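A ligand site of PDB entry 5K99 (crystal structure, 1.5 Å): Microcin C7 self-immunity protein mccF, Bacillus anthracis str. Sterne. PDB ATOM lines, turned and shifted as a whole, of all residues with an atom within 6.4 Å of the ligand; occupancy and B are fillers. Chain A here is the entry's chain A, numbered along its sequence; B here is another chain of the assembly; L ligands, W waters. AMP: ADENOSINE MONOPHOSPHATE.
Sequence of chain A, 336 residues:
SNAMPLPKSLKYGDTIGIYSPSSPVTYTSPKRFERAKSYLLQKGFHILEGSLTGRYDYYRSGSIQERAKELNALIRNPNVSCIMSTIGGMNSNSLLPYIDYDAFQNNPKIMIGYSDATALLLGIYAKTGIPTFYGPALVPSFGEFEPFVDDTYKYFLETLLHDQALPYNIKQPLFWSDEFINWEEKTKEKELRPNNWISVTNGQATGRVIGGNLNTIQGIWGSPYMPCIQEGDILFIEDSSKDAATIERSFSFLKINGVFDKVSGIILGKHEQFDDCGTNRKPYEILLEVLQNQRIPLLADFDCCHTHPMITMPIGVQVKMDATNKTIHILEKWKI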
ATOM      1  N   SER A  23       9.258 -28.115  17.857  1.00  0.00           N
ATOM      2  CA  SER A  23       9.771 -29.406  17.398  1.00  0.00           C
ATOM      3  C   SER A  23      10.442 -30.204  18.514  1.00  0.00           C
ATOM      4  O   SER A  23      11.108 -29.638  19.380  1.00  0.00           O
ATOM      5  CB  SER A  23      10.782 -29.213  16.281  1.00  0.00           C
ATOM      6  OG  SER A  23      10.195 -28.530  15.190  1.00  0.00           O
ATOM      7  N   VAL A  25      13.208 -31.809  19.154  1.00  0.00           N
ATOM      8  CA  VAL A  25      14.583 -32.049  18.750  1.00  0.00           C
ATOM      9  C   VAL A  25      15.337 -32.900  19.753  1.00  0.00           C
ATOM     10  O   VAL A  25      16.257 -33.632  19.375  1.00  0.00           O
ATOM     11  CB  VAL A  25      15.317 -30.708  18.494  1.00  0.00           C
ATOM     12  CG1 VAL A  25      15.512 -29.899  19.796  1.00  0.00           C
ATOM     13  CG2 VAL A  25      16.647 -30.939  17.814  1.00  0.00           C
ATOM     14  N   SER A  29      17.112 -35.495  17.361  1.00  0.00           N
ATOM     15  CA  SER A  29      18.548 -35.262  17.142  1.00  0.00           C
ATOM     16  C   SER A  29      19.272 -35.398  18.477  1.00  0.00           C
ATOM     17  O   SER A  29      19.819 -34.429  19.013  1.00  0.00           O
ATOM     18  CB  SER A  29      18.808 -33.895  16.507  1.00  0.00           C
ATOM     19  OG  SER A  29      18.405 -33.864  15.157  1.00  0.00           O
ATOM     20  N   ILE A  87      15.098 -25.557  20.257  1.00  0.00           N
ATOM     21  CA  ILE A  87      15.005 -25.365  18.828  1.00  0.00           C
ATOM     22  C   ILE A  87      13.659 -24.709  18.594  1.00  0.00           C
ATOM     23  O   ILE A  87      12.815 -24.658  19.494  1.00  0.00           O
ATOM     24  CB  ILE A  87      15.128 -26.699  18.063  1.00  0.00           C
ATOM     25  CG1 ILE A  87      15.481 -26.453  16.593  1.00  0.00           C
ATOM     26  CG2 ILE A  87      13.823 -27.473  18.169  1.00  0.00           C
ATOM     27  CD1 ILE A  87      16.160 -27.650  15.926  1.00  0.00           C
ATOM     28  N   GLY A  88      13.428 -24.228  17.377  1.00  0.00           N
ATOM     29  CA  GLY A  88      12.127 -23.713  16.970  1.00  0.00           C
ATOM     30  C   GLY A  88      11.247 -24.786  16.362  1.00  0.00           C
ATOM     31  O   GLY A  88      11.008 -25.829  16.969  1.00  0.00           O
ATOM     32  N   GLY A  89      10.742 -24.529  15.164  1.00  0.00           N
ATOM     33  CA  GLY A  89       9.724 -25.323  14.520  1.00  0.00           C
ATOM     34  C   GLY A  89       8.719 -24.412  13.858  1.00  0.00           C
ATOM     35  O   GLY A  89       9.102 -23.565  13.024  1.00  0.00           O
ATOM     36  N   MET A  90       7.442 -24.517  14.257  1.00  0.00           N
ATOM     37  CA  MET A  90       6.386 -23.644  13.760  1.00  0.00           C
ATOM     38  C   MET A  90       5.374 -23.206  14.808  1.00  0.00           C
ATOM     39  O   MET A  90       4.526 -22.331  14.521  1.00  0.00           O
ATOM     40  CB  MET A  90       5.596 -24.321  12.600  1.00  0.00           C
ATOM     41  CG  MET A  90       6.479 -24.679  11.431  1.00  0.00           C
ATOM     42  SD  MET A  90       5.495 -25.015   9.817  1.00  0.00           S
ATOM     43  CE  MET A  90       5.042 -23.158   9.453  1.00  0.00           C
ATOM     44  N   TYR A 114      15.822 -18.347  18.989  1.00  0.00           N
ATOM     45  CA  TYR A 114      15.624 -17.679  17.714  1.00  0.00           C
ATOM     46  C   TYR A 114      14.633 -18.457  16.842  1.00  0.00           C
ATOM     47  O   TYR A 114      13.955 -19.381  17.293  1.00  0.00           O
ATOM     48  CB  TYR A 114      16.975 -17.463  17.023  1.00  0.00           C
ATOM     49  CG  TYR A 114      17.650 -18.652  16.368  1.00  0.00           C
ATOM     50  CD1 TYR A 114      18.415 -19.565  17.082  1.00  0.00           C
ATOM     51  CD2 TYR A 114      17.578 -18.805  14.987  1.00  0.00           C
ATOM     52  CE1 TYR A 114      19.069 -20.627  16.451  1.00  0.00           C
ATOM     53  CE2 TYR A 114      18.189 -19.852  14.349  1.00  0.00           C
ATOM     54  CZ  TYR A 114      18.930 -20.753  15.082  1.00  0.00           C
ATOM     55  OH  TYR A 114      19.558 -21.793  14.394  1.00  0.00           O
ATOM     56  N   SER A 115      14.479 -18.003  15.599  1.00  0.00           N
ATOM     57  CA  SER A 115      13.598 -18.644  14.621  1.00  0.00           C
ATOM     58  C   SER A 115      12.180 -18.691  15.198  1.00  0.00           C
ATOM     59  O   SER A 115      11.645 -17.644  15.589  1.00  0.00           O
ATOM     60  CB  SER A 115      14.228 -19.990  14.264  1.00  0.00           C
ATOM     61  N   ASP A 116      11.500 -19.840  15.225  1.00  0.00           N
ATOM     62  CA  ASP A 116      10.118 -19.869  15.688  1.00  0.00           C
ATOM     63  C   ASP A 116       9.966 -19.329  17.119  1.00  0.00           C
ATOM     64  O   ASP A 116       8.882 -18.871  17.488  1.00  0.00           O
ATOM     65  CB  ASP A 116       9.590 -21.296  15.615  1.00  0.00           C
ATOM     66  CG  ASP A 116       8.112 -21.383  15.960  1.00  0.00           C
ATOM     67  OD1 ASP A 116       7.284 -20.804  15.206  1.00  0.00           O
ATOM     68  OD2 ASP A 116       7.800 -22.078  16.974  1.00  0.00           O
ATOM     69  N   ALA A 117      11.008 -19.406  17.952  1.00  0.00           N
ATOM     70  CA  ALA A 117      10.905 -18.879  19.310  1.00  0.00           C
ATOM     71  C   ALA A 117      10.682 -17.356  19.322  1.00  0.00           C
ATOM     72  O   ALA A 117      10.306 -16.812  20.375  1.00  0.00           O
ATOM     73  CB  ALA A 117      12.125 -19.268  20.135  1.00  0.00           C
ATOM     74  N   ALA A 137      19.771 -20.918  20.369  1.00  0.00           N
ATOM     75  CA  ALA A 137      18.946 -22.020  20.826  1.00  0.00           C
ATOM     76  C   ALA A 137      19.860 -23.217  21.074  1.00  0.00           C
ATOM     77  O   ALA A 137      20.886 -23.375  20.418  1.00  0.00           O
ATOM     78  CB  ALA A 137      17.858 -22.350  19.804  1.00  0.00           C
ATOM     79  N   PRO A 140      20.636 -26.173  17.867  1.00  0.00           N
ATOM     80  CA  PRO A 140      21.305 -25.640  16.667  1.00  0.00           C
ATOM     81  C   PRO A 140      22.571 -24.869  16.989  1.00  0.00           C
ATOM     82  O   PRO A 140      23.566 -24.999  16.287  1.00  0.00           O
ATOM     83  CB  PRO A 140      20.250 -24.729  16.014  1.00  0.00           C
ATOM     84  CG  PRO A 140      18.927 -25.163  16.603  1.00  0.00           C
ATOM     85  CD  PRO A 140      19.281 -25.632  18.029  1.00  0.00           C
ATOM     86  N   PHE A 180      25.264 -27.185   5.101  1.00  0.00           N
ATOM     87  CA  PHE A 180      24.281 -28.151   5.582  1.00  0.00           C
ATOM     88  C   PHE A 180      24.968 -29.510   5.831  1.00  0.00           C
ATOM     89  O   PHE A 180      24.701 -30.519   5.179  1.00  0.00           O
ATOM     90  CB  PHE A 180      23.125 -28.253   4.589  1.00  0.00           C
ATOM     91  CG  PHE A 180      21.900 -28.940   5.140  1.00  0.00           C
ATOM     92  CD1 PHE A 180      21.059 -28.276   5.993  1.00  0.00           C
ATOM     93  CD2 PHE A 180      21.582 -30.237   4.772  1.00  0.00           C
ATOM     94  CE1 PHE A 180      19.917 -28.898   6.503  1.00  0.00           C
ATOM     95  CE2 PHE A 180      20.453 -30.857   5.276  1.00  0.00           C
ATOM     96  CZ  PHE A 180      19.625 -30.183   6.144  1.00  0.00           C
ATOM     97  N   ILE A 181      25.913 -29.485   6.776  1.00  0.00           N
ATOM     98  CA  ILE A 181      26.661 -30.666   7.185  1.00  0.00           C
ATOM     99  C   ILE A 181      26.808 -30.665   8.707  1.00  0.00           C
ATOM    100  O   ILE A 181      26.458 -29.706   9.394  1.00  0.00           O
ATOM    101  CB  ILE A 181      28.062 -30.741   6.533  1.00  0.00           C
ATOM    102  CG1 ILE A 181      28.946 -29.591   7.021  1.00  0.00           C
ATOM    103  CG2 ILE A 181      27.934 -30.734   5.001  1.00  0.00           C
ATOM    104  CD1 ILE A 181      30.422 -29.718   6.595  1.00  0.00           C
ATOM    105  N   TRP A 183      25.465 -32.160  11.314  1.00  0.00           N
ATOM    106  CA  TRP A 183      24.338 -31.956  12.221  1.00  0.00           C
ATOM    107  C   TRP A 183      24.451 -32.869  13.442  1.00  0.00           C
ATOM    108  O   TRP A 183      24.682 -32.383  14.555  1.00  0.00           O
ATOM    109  CB  TRP A 183      23.004 -32.136  11.483  1.00  0.00           C
ATOM    110  CG  TRP A 183      21.816 -31.849  12.359  1.00  0.00           C
ATOM    111  CD1 TRP A 183      20.898 -32.743  12.815  1.00  0.00           C
ATOM    112  CD2 TRP A 183      21.442 -30.573  12.927  1.00  0.00           C
ATOM    113  NE1 TRP A 183      19.988 -32.120  13.636  1.00  0.00           N
ATOM    114  CE2 TRP A 183      20.291 -30.789  13.713  1.00  0.00           C
ATOM    115  CE3 TRP A 183      21.984 -29.290  12.862  1.00  0.00           C
ATOM    116  CZ2 TRP A 183      19.664 -29.763  14.402  1.00  0.00           C
ATOM    117  CZ3 TRP A 183      21.341 -28.266  13.547  1.00  0.00           C
ATOM    118  CH2 TRP A 183      20.199 -28.531  14.325  1.00  0.00           C
ATOM    119  N   SER A 240      15.674 -17.787   7.248  1.00  0.00           N
ATOM    120  CA  SER A 240      16.626 -18.853   7.063  1.00  0.00           C
ATOM    121  C   SER A 240      15.995 -20.001   6.290  1.00  0.00           C
ATOM    122  O   SER A 240      14.856 -20.381   6.573  1.00  0.00           O
ATOM    123  CB  SER A 240      17.103 -19.359   8.423  1.00  0.00           C
ATOM    124  OG  SER A 240      17.689 -18.337   9.219  1.00  0.00           O
ATOM    125  N   SER A 241      16.768 -20.574   5.355  1.00  0.00           N
ATOM    126  CA  SER A 241      16.376 -21.780   4.604  1.00  0.00           C
ATOM    127  C   SER A 241      14.998 -21.653   3.941  1.00  0.00           C
ATOM    128  O   SER A 241      14.220 -22.614   3.874  1.00  0.00           O
ATOM    129  CB  SER A 241      16.449 -23.009   5.491  1.00  0.00           C
ATOM    130  OG  SER A 241      17.797 -23.346   5.781  1.00  0.00           O
ATOM    131  N   GLU A 272      20.517 -18.227   5.499  1.00  0.00           N
ATOM    132  CA  GLU A 272      21.060 -19.569   5.382  1.00  0.00           C
ATOM    133  C   GLU A 272      20.468 -20.319   4.196  1.00  0.00           C
ATOM    134  O   GLU A 272      19.250 -20.425   4.063  1.00  0.00           O
ATOM    135  CB  GLU A 272      20.749 -20.323   6.663  1.00  0.00           C
ATOM    136  CG  GLU A 272      21.080 -21.833   6.618  1.00  0.00           C
ATOM    137  CD  GLU A 272      20.459 -22.580   7.728  1.00  0.00           C
ATOM    138  OE1 GLU A 272      19.245 -22.393   7.967  1.00  0.00           O
ATOM    139  OE2 GLU A 272      21.181 -23.367   8.389  1.00  0.00           O
ATOM    140  N   HIS A 306      20.423 -18.195  11.412  1.00  0.00           N
ATOM    141  CA  HIS A 306      20.802 -19.596  11.497  1.00  0.00           C
ATOM    142  C   HIS A 306      22.218 -19.886  11.008  1.00  0.00           C
ATOM    143  O   HIS A 306      22.724 -20.984  11.263  1.00  0.00           O
ATOM    144  CB  HIS A 306      19.821 -20.447  10.684  1.00  0.00           C
ATOM    145  N   THR A 307      22.869 -18.938  10.347  1.00  0.00           N
ATOM    146  CA  THR A 307      24.262 -19.131   9.962  1.00  0.00           C
ATOM    147  C   THR A 307      25.135 -19.108  11.217  1.00  0.00           C
ATOM    148  O   THR A 307      24.730 -18.618  12.278  1.00  0.00           O
ATOM    149  CB  THR A 307      24.715 -18.072   8.943  1.00  0.00           C
ATOM    150  OG1 THR A 307      24.673 -16.754   9.527  1.00  0.00           O
ATOM    151  CG2 THR A 307      23.801 -18.076   7.724  1.00  0.00           C
ATOM    152  N   HIS A 308      26.345 -19.680  11.105  1.00  0.00           N
ATOM    153  CA  HIS A 308      27.287 -19.745  12.203  1.00  0.00           C
ATOM    154  C   HIS A 308      28.446 -18.803  11.938  1.00  0.00           C
ATOM    155  O   HIS A 308      28.980 -18.826  10.853  1.00  0.00           O
ATOM    156  CB  HIS A 308      27.819 -21.165  12.414  1.00  0.00           C
ATOM    157  CG  HIS A 308      26.731 -22.145  12.710  1.00  0.00           C
ATOM    158  ND1 HIS A 308      26.247 -22.367  13.980  1.00  0.00           N
ATOM    159  CD2 HIS A 308      25.998 -22.918  11.886  1.00  0.00           C
ATOM    160  CE1 HIS A 308      25.254 -23.237  13.921  1.00  0.00           C
ATOM    161  NE2 HIS A 308      25.089 -23.594  12.668  1.00  0.00           N
ATOM    162  N   ARG B   2      16.286 -29.872   4.890  1.00  0.00           N
ATOM    163  CA  ARG B   2      15.116 -30.497   5.497  1.00  0.00           C
ATOM    164  C   ARG B   2      13.971 -30.422   4.543  1.00  0.00           C
ATOM    165  O   ARG B   2      13.932 -29.513   3.727  1.00  0.00           O
ATOM    166  CB  ARG B   2      14.694 -29.826   6.812  1.00  0.00           C
ATOM    167  CG  ARG B   2      15.855 -29.618   7.789  1.00  0.00           C
ATOM    168  CD  ARG B   2      15.621 -28.413   8.679  1.00  0.00           C
ATOM    169  NE  ARG B   2      14.726 -28.860   9.729  1.00  0.00           N
ATOM    170  CZ  ARG B   2      14.135 -28.097  10.655  1.00  0.00           C
ATOM    171  NH1 ARG B   2      14.287 -26.753  10.725  1.00  0.00           N
ATOM    172  NH2 ARG B   2      13.359 -28.697  11.537  1.00  0.00           N
ATOM    173  N   ALA B   6       9.977 -25.447   8.502  1.00  0.00           N
ATOM    174  CA  ALA B   6      10.149 -24.898   9.825  1.00  0.00           C
ATOM    175  C   ALA B   6      11.133 -23.762   9.918  1.00  0.00           C
ATOM    176  O   ALA B   6      12.000 -23.577   9.065  1.00  0.00           O
ATOM    177  CB  ALA B   6      10.660 -26.029  10.700  1.00  0.00           C
ATOM    178  C   XSN B   7      12.525 -22.485  12.637  1.00  0.00           C
ATOM    179  N   XSN B   7      10.953 -22.972  10.993  1.00  0.00           N
ATOM    180  O   XSN B   7      11.992 -22.389  13.745  1.00  0.00           O
ATOM    181  CA  XSN B   7      11.868 -21.882  11.390  1.00  0.00           C
ATOM    182  CB  XSN B   7      11.085 -20.607  11.654  1.00  0.00           C
ATOM    183  CG  XSN B   7      10.404 -20.123  10.388  1.00  0.00           C
ATOM    184  OD1 XSN B   7      11.092 -19.997   9.364  1.00  0.00           O
ATOM    185  OD2 XSN B   7       9.173 -19.888  10.433  1.00  0.00           O
ATOM    186  N1  XSN B   7      13.659 -23.185  12.398  1.00  0.00           N
HETATM  187  P   AMP L   1      14.426 -24.172  13.565  1.00  0.00           P
HETATM  188  O1P AMP L   1      14.578 -23.483  14.878  1.00  0.00           O
HETATM  189  O2P AMP L   1      13.685 -25.452  13.481  1.00  0.00           O
HETATM  190  O5' AMP L   1      15.841 -24.418  12.897  1.00  0.00           O
HETATM  191  C5' AMP L   1      16.899 -23.457  13.103  1.00  0.00           C
HETATM  192  C4' AMP L   1      18.125 -23.950  12.357  1.00  0.00           C
HETATM  193  O4' AMP L   1      18.576 -25.226  12.841  1.00  0.00           O
HETATM  194  C3' AMP L   1      17.865 -24.236  10.894  1.00  0.00           C
HETATM  195  O3' AMP L   1      17.693 -23.064  10.107  1.00  0.00           O
HETATM  196  C2' AMP L   1      19.070 -25.069  10.546  1.00  0.00           C
HETATM  197  O2' AMP L   1      20.278 -24.279  10.563  1.00  0.00           O
HETATM  198  C1' AMP L   1      19.118 -25.978  11.760  1.00  0.00           C
HETATM  199  N9  AMP L   1      18.429 -27.284  11.702  1.00  0.00           N
HETATM  200  C8  AMP L   1      17.299 -27.594  12.329  1.00  0.00           C
HETATM  201  N7  AMP L   1      17.005 -28.884  12.113  1.00  0.00           N
HETATM  202  C5  AMP L   1      17.971 -29.389  11.330  1.00  0.00           C
HETATM  203  C6  AMP L   1      18.213 -30.654  10.780  1.00  0.00           C
HETATM  204  N6  AMP L   1      17.354 -31.677  11.024  1.00  0.00           N
HETATM  205  N1  AMP L   1      19.317 -30.808  10.018  1.00  0.00           N
HETATM  206  C2  AMP L   1      20.181 -29.790   9.805  1.00  0.00           C
HETATM  207  N3  AMP L   1      19.962 -28.560  10.307  1.00  0.00           N
HETATM  208  C4  AMP L   1      18.872 -28.376  11.072  1.00  0.00           C
HETATM  209  O   HOH W   1      23.500 -29.519   9.033  1.00  0.00           O
HETATM  210  O   HOH W   2      12.587 -27.763  14.115  1.00  0.00           O
HETATM  211  O   HOH W   3      16.249 -22.492  16.755  1.00  0.00           O
HETATM  212  O   HOH W   4      20.345 -33.020   8.781  1.00  0.00           O
HETATM  213  O   HOH W   5      15.085 -22.648   9.839  1.00  0.00           O
HETATM  214  O   HOH W   6      17.519 -34.722  10.766  1.00  0.00           O
HETATM  215  O   HOH W   7      15.703 -30.843  13.659  1.00  0.00           O
HETATM  216  O   HOH W   8      22.280 -27.157   9.265  1.00  0.00           O
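The backbone carbonyl oxygen of Gly 89 sits at hydrogen-bond distance from N of XSN 7 of chain B (2.8 Å). The backbone NH (N) of Asp 116 lies within hydrogen-bond range of O of XSN 7 of chain B, 3.0 Å away. OE1 of Glu 272 is in hydrogen-bond range of OG of Ser 241 (2.8 Å). N of Ser 23 is in hydrogen-bond range of O of Gly 88, 3.0 Å away. The side-chain hydroxyl of Ser 29 sits at hydrogen-bond distance from the indole nitrogen of Trp 183 (2.8 Å).
Water W2 lies within hydrogen-bond range of O2P of the ligand (2.6 Å), OG of Ser 23 (2.7 Å) and NH2 of Arg 2 of chain B (2.8 Å). Water W5 lies within hydrogen-bond range of an oxygen (O3') of the ligand (2.7 Å), N1 of XSN 7 of chain B (3.0 Å) and the backbone carbonyl oxygen (O) of Ala 6 of chain B (3.3 Å). Water W3 lies within hydrogen-bond range of an oxygen (O1P) of the ligand (2.7 Å) and the backbone NH (N) of Gly 88 (3.4 Å).
Residues that only touch the ligand: Ile 87 (3.5 Å), Gly 89 (3.5 Å), Tyr 114 (3.3 Å), Ser 115 (3.6 Å), Pro 140 (3.6 Å), Phe 180 (3.4 Å), Trp 183 (3.3 Å) and His 306 (3.4 Å). Within 4 Å of the ligand: Ile 87, Gly 88, Gly 89, Tyr 114, Ser 115, Pro 140, Phe 180, Trp 183, Glu 272, His 306, Arg 2 of chain B and XSN 7 of chain B.
O of XSN 7 of chain B lies close to O1P of the ligand, at 3.0 Å. P of the ligand is covalently linked to N1 of XSN 7 of chain B, at 1.7 Å. OE2 of Glu 272 sits at hydrogen-bond distance from O2' of the ligand (2.5 Å). N of Gly 88 is in hydrogen-bond range of O1P of the ligand (2.9 Å). NH1 of Arg 2 of chain B lies within salt-bridge range of O2P of the ligand (3.1 Å).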
